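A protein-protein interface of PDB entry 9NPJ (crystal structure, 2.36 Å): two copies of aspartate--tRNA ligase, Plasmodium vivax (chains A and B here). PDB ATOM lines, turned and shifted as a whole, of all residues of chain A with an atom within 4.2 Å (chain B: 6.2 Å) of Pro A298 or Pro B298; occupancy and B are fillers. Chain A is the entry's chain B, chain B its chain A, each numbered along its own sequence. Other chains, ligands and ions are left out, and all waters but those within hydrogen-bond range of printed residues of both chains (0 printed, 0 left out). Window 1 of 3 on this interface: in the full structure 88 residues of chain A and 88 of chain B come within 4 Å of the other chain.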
ATOM      1  N   LYS A 250     -28.076 -11.727  11.552  1.00  0.00           N
ATOM      2  CA  LYS A 250     -28.353 -11.673  12.981  1.00  0.00           C
ATOM      3  C   LYS A 250     -29.210 -10.470  13.373  1.00  0.00           C
ATOM      4  O   LYS A 250     -29.678 -10.417  14.521  1.00  0.00           O
ATOM      5  CB  LYS A 250     -27.041 -11.665  13.783  1.00  0.00           C
ATOM      6  CG  LYS A 250     -25.995 -12.637  13.246  1.00  0.00           C
ATOM      7  CD  LYS A 250     -26.509 -14.079  13.192  1.00  0.00           C
ATOM      8  CE  LYS A 250     -25.507 -14.968  12.447  1.00  0.00           C
ATOM      9  NZ  LYS A 250     -26.158 -16.109  11.749  1.00  0.00           N
ATOM     10  N   ALA A 297     -21.554 -19.388  13.619  1.00  0.00           N
ATOM     11  CA  ALA A 297     -21.812 -17.965  13.757  1.00  0.00           C
ATOM     12  C   ALA A 297     -22.290 -17.675  15.165  1.00  0.00           C
ATOM     13  O   ALA A 297     -22.855 -18.559  15.835  1.00  0.00           O
ATOM     14  CB  ALA A 297     -22.852 -17.478  12.730  1.00  0.00           C
ATOM     15  N   PRO A 298     -22.110 -16.458  15.649  1.00  0.00           N
ATOM     16  CA  PRO A 298     -22.616 -16.088  16.969  1.00  0.00           C
ATOM     17  C   PRO A 298     -24.136 -16.018  17.002  1.00  0.00           C
ATOM     18  O   PRO A 298     -24.796 -15.797  15.986  1.00  0.00           O
ATOM     19  CB  PRO A 298     -22.002 -14.705  17.214  1.00  0.00           C
ATOM     20  CG  PRO A 298     -21.685 -14.186  15.855  1.00  0.00           C
ATOM     21  CD  PRO A 298     -21.324 -15.378  15.016  1.00  0.00           C
ATOM     22  N   VAL A 299     -24.687 -16.243  18.196  1.00  0.00           N
ATOM     23  CA  VAL A 299     -26.087 -15.972  18.495  1.00  0.00           C
ATOM     24  C   VAL A 299     -26.129 -15.184  19.801  1.00  0.00           C
ATOM     25  O   VAL A 299     -25.151 -15.127  20.551  1.00  0.00           O
ATOM     26  CB  VAL A 299     -26.930 -17.261  18.592  1.00  0.00           C
ATOM     27  CG1 VAL A 299     -26.892 -18.004  17.264  1.00  0.00           C
ATOM     28  CG2 VAL A 299     -26.442 -18.169  19.764  1.00  0.00           C
ATOM     29  N   PHE A 300     -27.280 -14.572  20.073  1.00  0.00           N
ATOM     30  CA  PHE A 300     -27.404 -13.608  21.164  1.00  0.00           C
ATOM     31  C   PHE A 300     -28.657 -13.922  21.963  1.00  0.00           C
ATOM     32  O   PHE A 300     -29.765 -13.946  21.408  1.00  0.00           O
ATOM     33  CB  PHE A 300     -27.443 -12.177  20.614  1.00  0.00           C
ATOM     34  CG  PHE A 300     -26.337 -11.884  19.632  1.00  0.00           C
ATOM     35  CD1 PHE A 300     -26.508 -12.131  18.286  1.00  0.00           C
ATOM     36  CD2 PHE A 300     -25.111 -11.390  20.066  1.00  0.00           C
ATOM     37  CE1 PHE A 300     -25.486 -11.870  17.375  1.00  0.00           C
ATOM     38  CE2 PHE A 300     -24.067 -11.133  19.161  1.00  0.00           C
ATOM     39  CZ  PHE A 300     -24.254 -11.370  17.815  1.00  0.00           C
ATOM     40  N   GLU A 313     -23.895 -14.483  24.801  1.00  0.00           N
ATOM     41  CA  GLU A 313     -23.406 -14.612  23.444  1.00  0.00           C
ATOM     42  C   GLU A 313     -22.555 -15.873  23.404  1.00  0.00           C
ATOM     43  O   GLU A 313     -21.736 -16.106  24.306  1.00  0.00           O
ATOM     44  CB  GLU A 313     -22.595 -13.378  23.017  1.00  0.00           C
ATOM     45  CG  GLU A 313     -22.095 -13.462  21.586  1.00  0.00           C
ATOM     46  CD  GLU A 313     -21.343 -12.213  21.127  1.00  0.00           C
ATOM     47  OE1 GLU A 313     -21.314 -11.204  21.890  1.00  0.00           O
ATOM     48  OE2 GLU A 313     -20.786 -12.245  19.994  1.00  0.00           O
ATOM     49  N   TYR A 314     -22.780 -16.699  22.390  1.00  0.00           N
ATOM     50  CA  TYR A 314     -22.004 -17.914  22.213  1.00  0.00           C
ATOM     51  C   TYR A 314     -21.980 -18.225  20.727  1.00  0.00           C
ATOM     52  O   TYR A 314     -22.735 -17.646  19.939  1.00  0.00           O
ATOM     53  CB  TYR A 314     -22.574 -19.068  23.051  1.00  0.00           C
ATOM     54  CG  TYR A 314     -23.868 -19.694  22.569  1.00  0.00           C
ATOM     55  CD1 TYR A 314     -25.103 -19.231  23.019  1.00  0.00           C
ATOM     56  CD2 TYR A 314     -23.851 -20.789  21.696  1.00  0.00           C
ATOM     57  CE1 TYR A 314     -26.290 -19.823  22.588  1.00  0.00           C
ATOM     58  CE2 TYR A 314     -25.028 -21.391  21.252  1.00  0.00           C
ATOM     59  CZ  TYR A 314     -26.241 -20.914  21.701  1.00  0.00           C
ATOM     60  OH  TYR A 314     -27.407 -21.509  21.261  1.00  0.00           O
ATOM     61  N   HIS B 247     -13.128 -16.744  17.878  1.00  0.00           N
ATOM     62  CA  HIS B 247     -14.461 -16.167  17.891  1.00  0.00           C
ATOM     63  C   HIS B 247     -14.467 -15.108  18.974  1.00  0.00           C
ATOM     64  O   HIS B 247     -14.234 -15.415  20.147  1.00  0.00           O
ATOM     65  CB  HIS B 247     -15.538 -17.233  18.133  1.00  0.00           C
ATOM     66  CG  HIS B 247     -15.535 -18.321  17.100  1.00  0.00           C
ATOM     67  ND1 HIS B 247     -16.203 -18.210  15.900  1.00  0.00           N
ATOM     68  CD2 HIS B 247     -14.895 -19.512  17.063  1.00  0.00           C
ATOM     69  CE1 HIS B 247     -15.995 -19.296  15.178  1.00  0.00           C
ATOM     70  NE2 HIS B 247     -15.206 -20.106  15.861  1.00  0.00           N
ATOM     71  N   THR B 248     -14.709 -13.869  18.579  1.00  0.00           N
ATOM     72  CA  THR B 248     -14.707 -12.746  19.497  1.00  0.00           C
ATOM     73  C   THR B 248     -16.082 -12.089  19.520  1.00  0.00           C
ATOM     74  O   THR B 248     -16.842 -12.192  18.551  1.00  0.00           O
ATOM     75  CB  THR B 248     -13.621 -11.739  19.092  1.00  0.00           C
ATOM     76  OG1 THR B 248     -13.938 -11.166  17.815  1.00  0.00           O
ATOM     77  CG2 THR B 248     -12.278 -12.454  19.000  1.00  0.00           C
ATOM     78  N   LYS B 250     -19.573  -9.831  19.609  1.00  0.00           N
ATOM     79  CA  LYS B 250     -20.158  -8.754  18.830  1.00  0.00           C
ATOM     80  C   LYS B 250     -20.939  -7.756  19.677  1.00  0.00           C
ATOM     81  O   LYS B 250     -21.227  -6.652  19.197  1.00  0.00           O
ATOM     82  CB  LYS B 250     -21.077  -9.316  17.739  1.00  0.00           C
ATOM     83  CG  LYS B 250     -20.460 -10.446  16.932  1.00  0.00           C
ATOM     84  CD  LYS B 250     -19.070 -10.102  16.459  1.00  0.00           C
ATOM     85  CE  LYS B 250     -18.450 -11.281  15.709  1.00  0.00           C
ATOM     86  NZ  LYS B 250     -16.963 -11.239  15.807  1.00  0.00           N
ATOM     87  N   ALA B 275     -20.547  -4.755  17.253  1.00  0.00           N
ATOM     88  CA  ALA B 275     -19.209  -4.654  16.685  1.00  0.00           C
ATOM     89  C   ALA B 275     -19.273  -4.300  15.201  1.00  0.00           C
ATOM     90  O   ALA B 275     -19.964  -4.953  14.413  1.00  0.00           O
ATOM     91  CB  ALA B 275     -18.453  -5.969  16.884  1.00  0.00           C
ATOM     92  N   PRO B 278     -13.971  -7.017  14.355  1.00  0.00           N
ATOM     93  CA  PRO B 278     -13.287  -7.622  15.502  1.00  0.00           C
ATOM     94  C   PRO B 278     -11.929  -7.015  15.806  1.00  0.00           C
ATOM     95  O   PRO B 278     -11.193  -7.580  16.622  1.00  0.00           O
ATOM     96  CB  PRO B 278     -13.134  -9.085  15.068  1.00  0.00           C
ATOM     97  CG  PRO B 278     -12.954  -8.978  13.568  1.00  0.00           C
ATOM     98  CD  PRO B 278     -13.822  -7.818  13.122  1.00  0.00           C
ATOM     99  N   VAL B 296     -14.022 -15.599  10.923  1.00  0.00           N
ATOM    100  CA  VAL B 296     -15.070 -15.480   9.916  1.00  0.00           C
ATOM    101  C   VAL B 296     -16.368 -15.247  10.669  1.00  0.00           C
ATOM    102  O   VAL B 296     -16.899 -16.177  11.291  1.00  0.00           O
ATOM    103  CB  VAL B 296     -15.178 -16.739   9.048  1.00  0.00           C
ATOM    104  CG1 VAL B 296     -16.300 -16.569   8.004  1.00  0.00           C
ATOM    105  CG2 VAL B 296     -13.834 -17.084   8.409  1.00  0.00           C
ATOM    106  N   ALA B 297     -16.895 -14.029  10.625  1.00  0.00           N
ATOM    107  CA  ALA B 297     -18.039 -13.719  11.469  1.00  0.00           C
ATOM    108  C   ALA B 297     -18.736 -12.483  10.932  1.00  0.00           C
ATOM    109  O   ALA B 297     -18.118 -11.668  10.231  1.00  0.00           O
ATOM    110  CB  ALA B 297     -17.610 -13.508  12.938  1.00  0.00           C
ATOM    111  N   PRO B 298     -20.014 -12.297  11.258  1.00  0.00           N
ATOM    112  CA  PRO B 298     -20.706 -11.060  10.886  1.00  0.00           C
ATOM    113  C   PRO B 298     -20.144  -9.847  11.612  1.00  0.00           C
ATOM    114  O   PRO B 298     -19.592  -9.954  12.711  1.00  0.00           O
ATOM    115  CB  PRO B 298     -22.158 -11.321  11.307  1.00  0.00           C
ATOM    116  CG  PRO B 298     -22.105 -12.428  12.276  1.00  0.00           C
ATOM    117  CD  PRO B 298     -20.912 -13.264  11.926  1.00  0.00           C
ATOM    118  N   VAL B 299     -20.271  -8.686  10.955  1.00  0.00           N
ATOM    119  CA  VAL B 299     -20.118  -7.372  11.568  1.00  0.00           C
ATOM    120  C   VAL B 299     -21.336  -6.527  11.180  1.00  0.00           C
ATOM    121  O   VAL B 299     -22.073  -6.845  10.245  1.00  0.00           O
ATOM    122  CB  VAL B 299     -18.802  -6.663  11.158  1.00  0.00           C
ATOM    123  CG1 VAL B 299     -17.595  -7.478  11.577  1.00  0.00           C
ATOM    124  CG2 VAL B 299     -18.768  -6.366   9.651  1.00  0.00           C
ATOM    125  N   PHE B 300     -21.543  -5.438  11.910  1.00  0.00           N
ATOM    126  CA  PHE B 300     -22.774  -4.661  11.807  1.00  0.00           C
ATOM    127  C   PHE B 300     -22.428  -3.186  11.673  1.00  0.00           C
ATOM    128  O   PHE B 300     -21.778  -2.619  12.554  1.00  0.00           O
ATOM    129  CB  PHE B 300     -23.663  -4.913  13.025  1.00  0.00           C
ATOM    130  CG  PHE B 300     -23.827  -6.366  13.336  1.00  0.00           C
ATOM    131  CD1 PHE B 300     -22.927  -7.012  14.189  1.00  0.00           C
ATOM    132  CD2 PHE B 300     -24.854  -7.107  12.744  1.00  0.00           C
ATOM    133  CE1 PHE B 300     -23.061  -8.367  14.472  1.00  0.00           C
ATOM    134  CE2 PHE B 300     -24.994  -8.462  13.015  1.00  0.00           C
ATOM    135  CZ  PHE B 300     -24.092  -9.097  13.884  1.00  0.00           C
ATOM    136  N   GLU B 313     -25.076  -5.279   7.307  1.00  0.00           N
ATOM    137  CA  GLU B 313     -24.557  -6.478   7.937  1.00  0.00           C
ATOM    138  C   GLU B 313     -23.838  -7.265   6.856  1.00  0.00           C
ATOM    139  O   GLU B 313     -24.374  -7.431   5.761  1.00  0.00           O
ATOM    140  CB  GLU B 313     -25.686  -7.317   8.551  1.00  0.00           C
ATOM    141  CG  GLU B 313     -25.203  -8.555   9.297  1.00  0.00           C
ATOM    142  CD  GLU B 313     -26.341  -9.377   9.927  1.00  0.00           C
ATOM    143  OE1 GLU B 313     -27.533  -8.947   9.898  1.00  0.00           O
ATOM    144  OE2 GLU B 313     -26.021 -10.464  10.463  1.00  0.00           O
ATOM    145  N   TYR B 314     -22.633  -7.740   7.145  1.00  0.00           N
ATOM    146  CA  TYR B 314     -21.931  -8.567   6.178  1.00  0.00           C
ATOM    147  C   TYR B 314     -20.950  -9.460   6.924  1.00  0.00           C
ATOM    148  O   TYR B 314     -20.644  -9.235   8.099  1.00  0.00           O
ATOM    149  CB  TYR B 314     -21.217  -7.714   5.109  1.00  0.00           C
ATOM    150  CG  TYR B 314     -19.977  -6.978   5.591  1.00  0.00           C
ATOM    151  CD1 TYR B 314     -20.058  -5.677   6.097  1.00  0.00           C
ATOM    152  CD2 TYR B 314     -18.726  -7.585   5.536  1.00  0.00           C
ATOM    153  CE1 TYR B 314     -18.916  -5.001   6.529  1.00  0.00           C
ATOM    154  CE2 TYR B 314     -17.587  -6.923   5.946  1.00  0.00           C
ATOM    155  CZ  TYR B 314     -17.671  -5.629   6.448  1.00  0.00           C
ATOM    156  OH  TYR B 314     -16.505  -4.985   6.874  1.00  0.00           O
ATOM    157  N   VAL B 315     -20.462 -10.481   6.223  1.00  0.00           N
ATOM    158  CA  VAL B 315     -19.491 -11.424   6.771  1.00  0.00           C
ATOM    159  C   VAL B 315     -18.082 -10.874   6.560  1.00  0.00           C
ATOM    160  O   VAL B 315     -17.640 -10.664   5.421  1.00  0.00           O
ATOM    161  CB  VAL B 315     -19.646 -12.806   6.123  1.00  0.00           C
ATOM    162  CG1 VAL B 315     -18.611 -13.794   6.705  1.00  0.00           C
ATOM    163  CG2 VAL B 315     -21.058 -13.314   6.337  1.00  0.00           C
ATOM    164  N   SER B 316     -17.371 -10.634   7.652  1.00  0.00           N
ATOM    165  CA  SER B 316     -16.011 -10.132   7.583  1.00  0.00           C
ATOM    166  C   SER B 316     -15.009 -11.270   7.770  1.00  0.00           C
ATOM    167  O   SER B 316     -15.157 -12.099   8.675  1.00  0.00           O
ATOM    168  CB  SER B 316     -15.776  -9.051   8.633  1.00  0.00           C
ATOM    169  OG  SER B 316     -14.404  -8.655   8.604  1.00  0.00           O
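Of the 14 printed residues of chain B, 4 touch a printed residue of chain A. Printed residues of chain A that touch a printed residue of chain B: Lys A250, Pro A298, Phe A300 and Glu A313.
OE2 of Glu A313 lies within hydrogen-bond range of N of Lys B250 (2.7 Å). The backbone NH (N) of Lys A250 lies within hydrogen-bond range of the side-chain carboxylate (OE2) of Glu B313 (2.6 Å).
The backbone carbonyl oxygen (O) of Ala B275 lies within hydrogen-bond range of the backbone NH (N) of Phe B300. O of Thr B248 sits at hydrogen-bond distance from NZ of Lys B250 (2.9 Å). O of Lys B250 sits at hydrogen-bond distance from N of Ala B275 (2.8 Å).
Among the printed residues, merely in contact across the chains: Pro A298 with Pro B298 (3.8 Å), Phe A300 with Lys B250 (3.8 Å) and Lys A250 with Phe B300 (3.9 Å).
Pro A298 touches just one residue of chain B: Pro B298. Of the printed residues of chain A, Pro B298 touches Pro A298. Of the printed residues of chain B, Phe A300 touches Lys B250. Of the printed residues of chain A, Glu B313 touches Lys A250 (2.6 Å). Ala B297 touches none of the printed residues of chain A. His B247 touches none of the printed residues of chain A. The nearest residue of chain B that does not touch Pro A298 is Lys B250 (4.1 Å). The nearest printed residue of chain B that does not touch Phe A300 is Phe B300 (4.5 Å).
Lys A250 touches Phe B300, and with the chains exchanged Phe A300 touches Lys B250. Lys A250 touches Glu B313, and with the chains exchanged Glu A313 touches Lys B250. Pro A298 touches its own counterpart, Pro B298.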
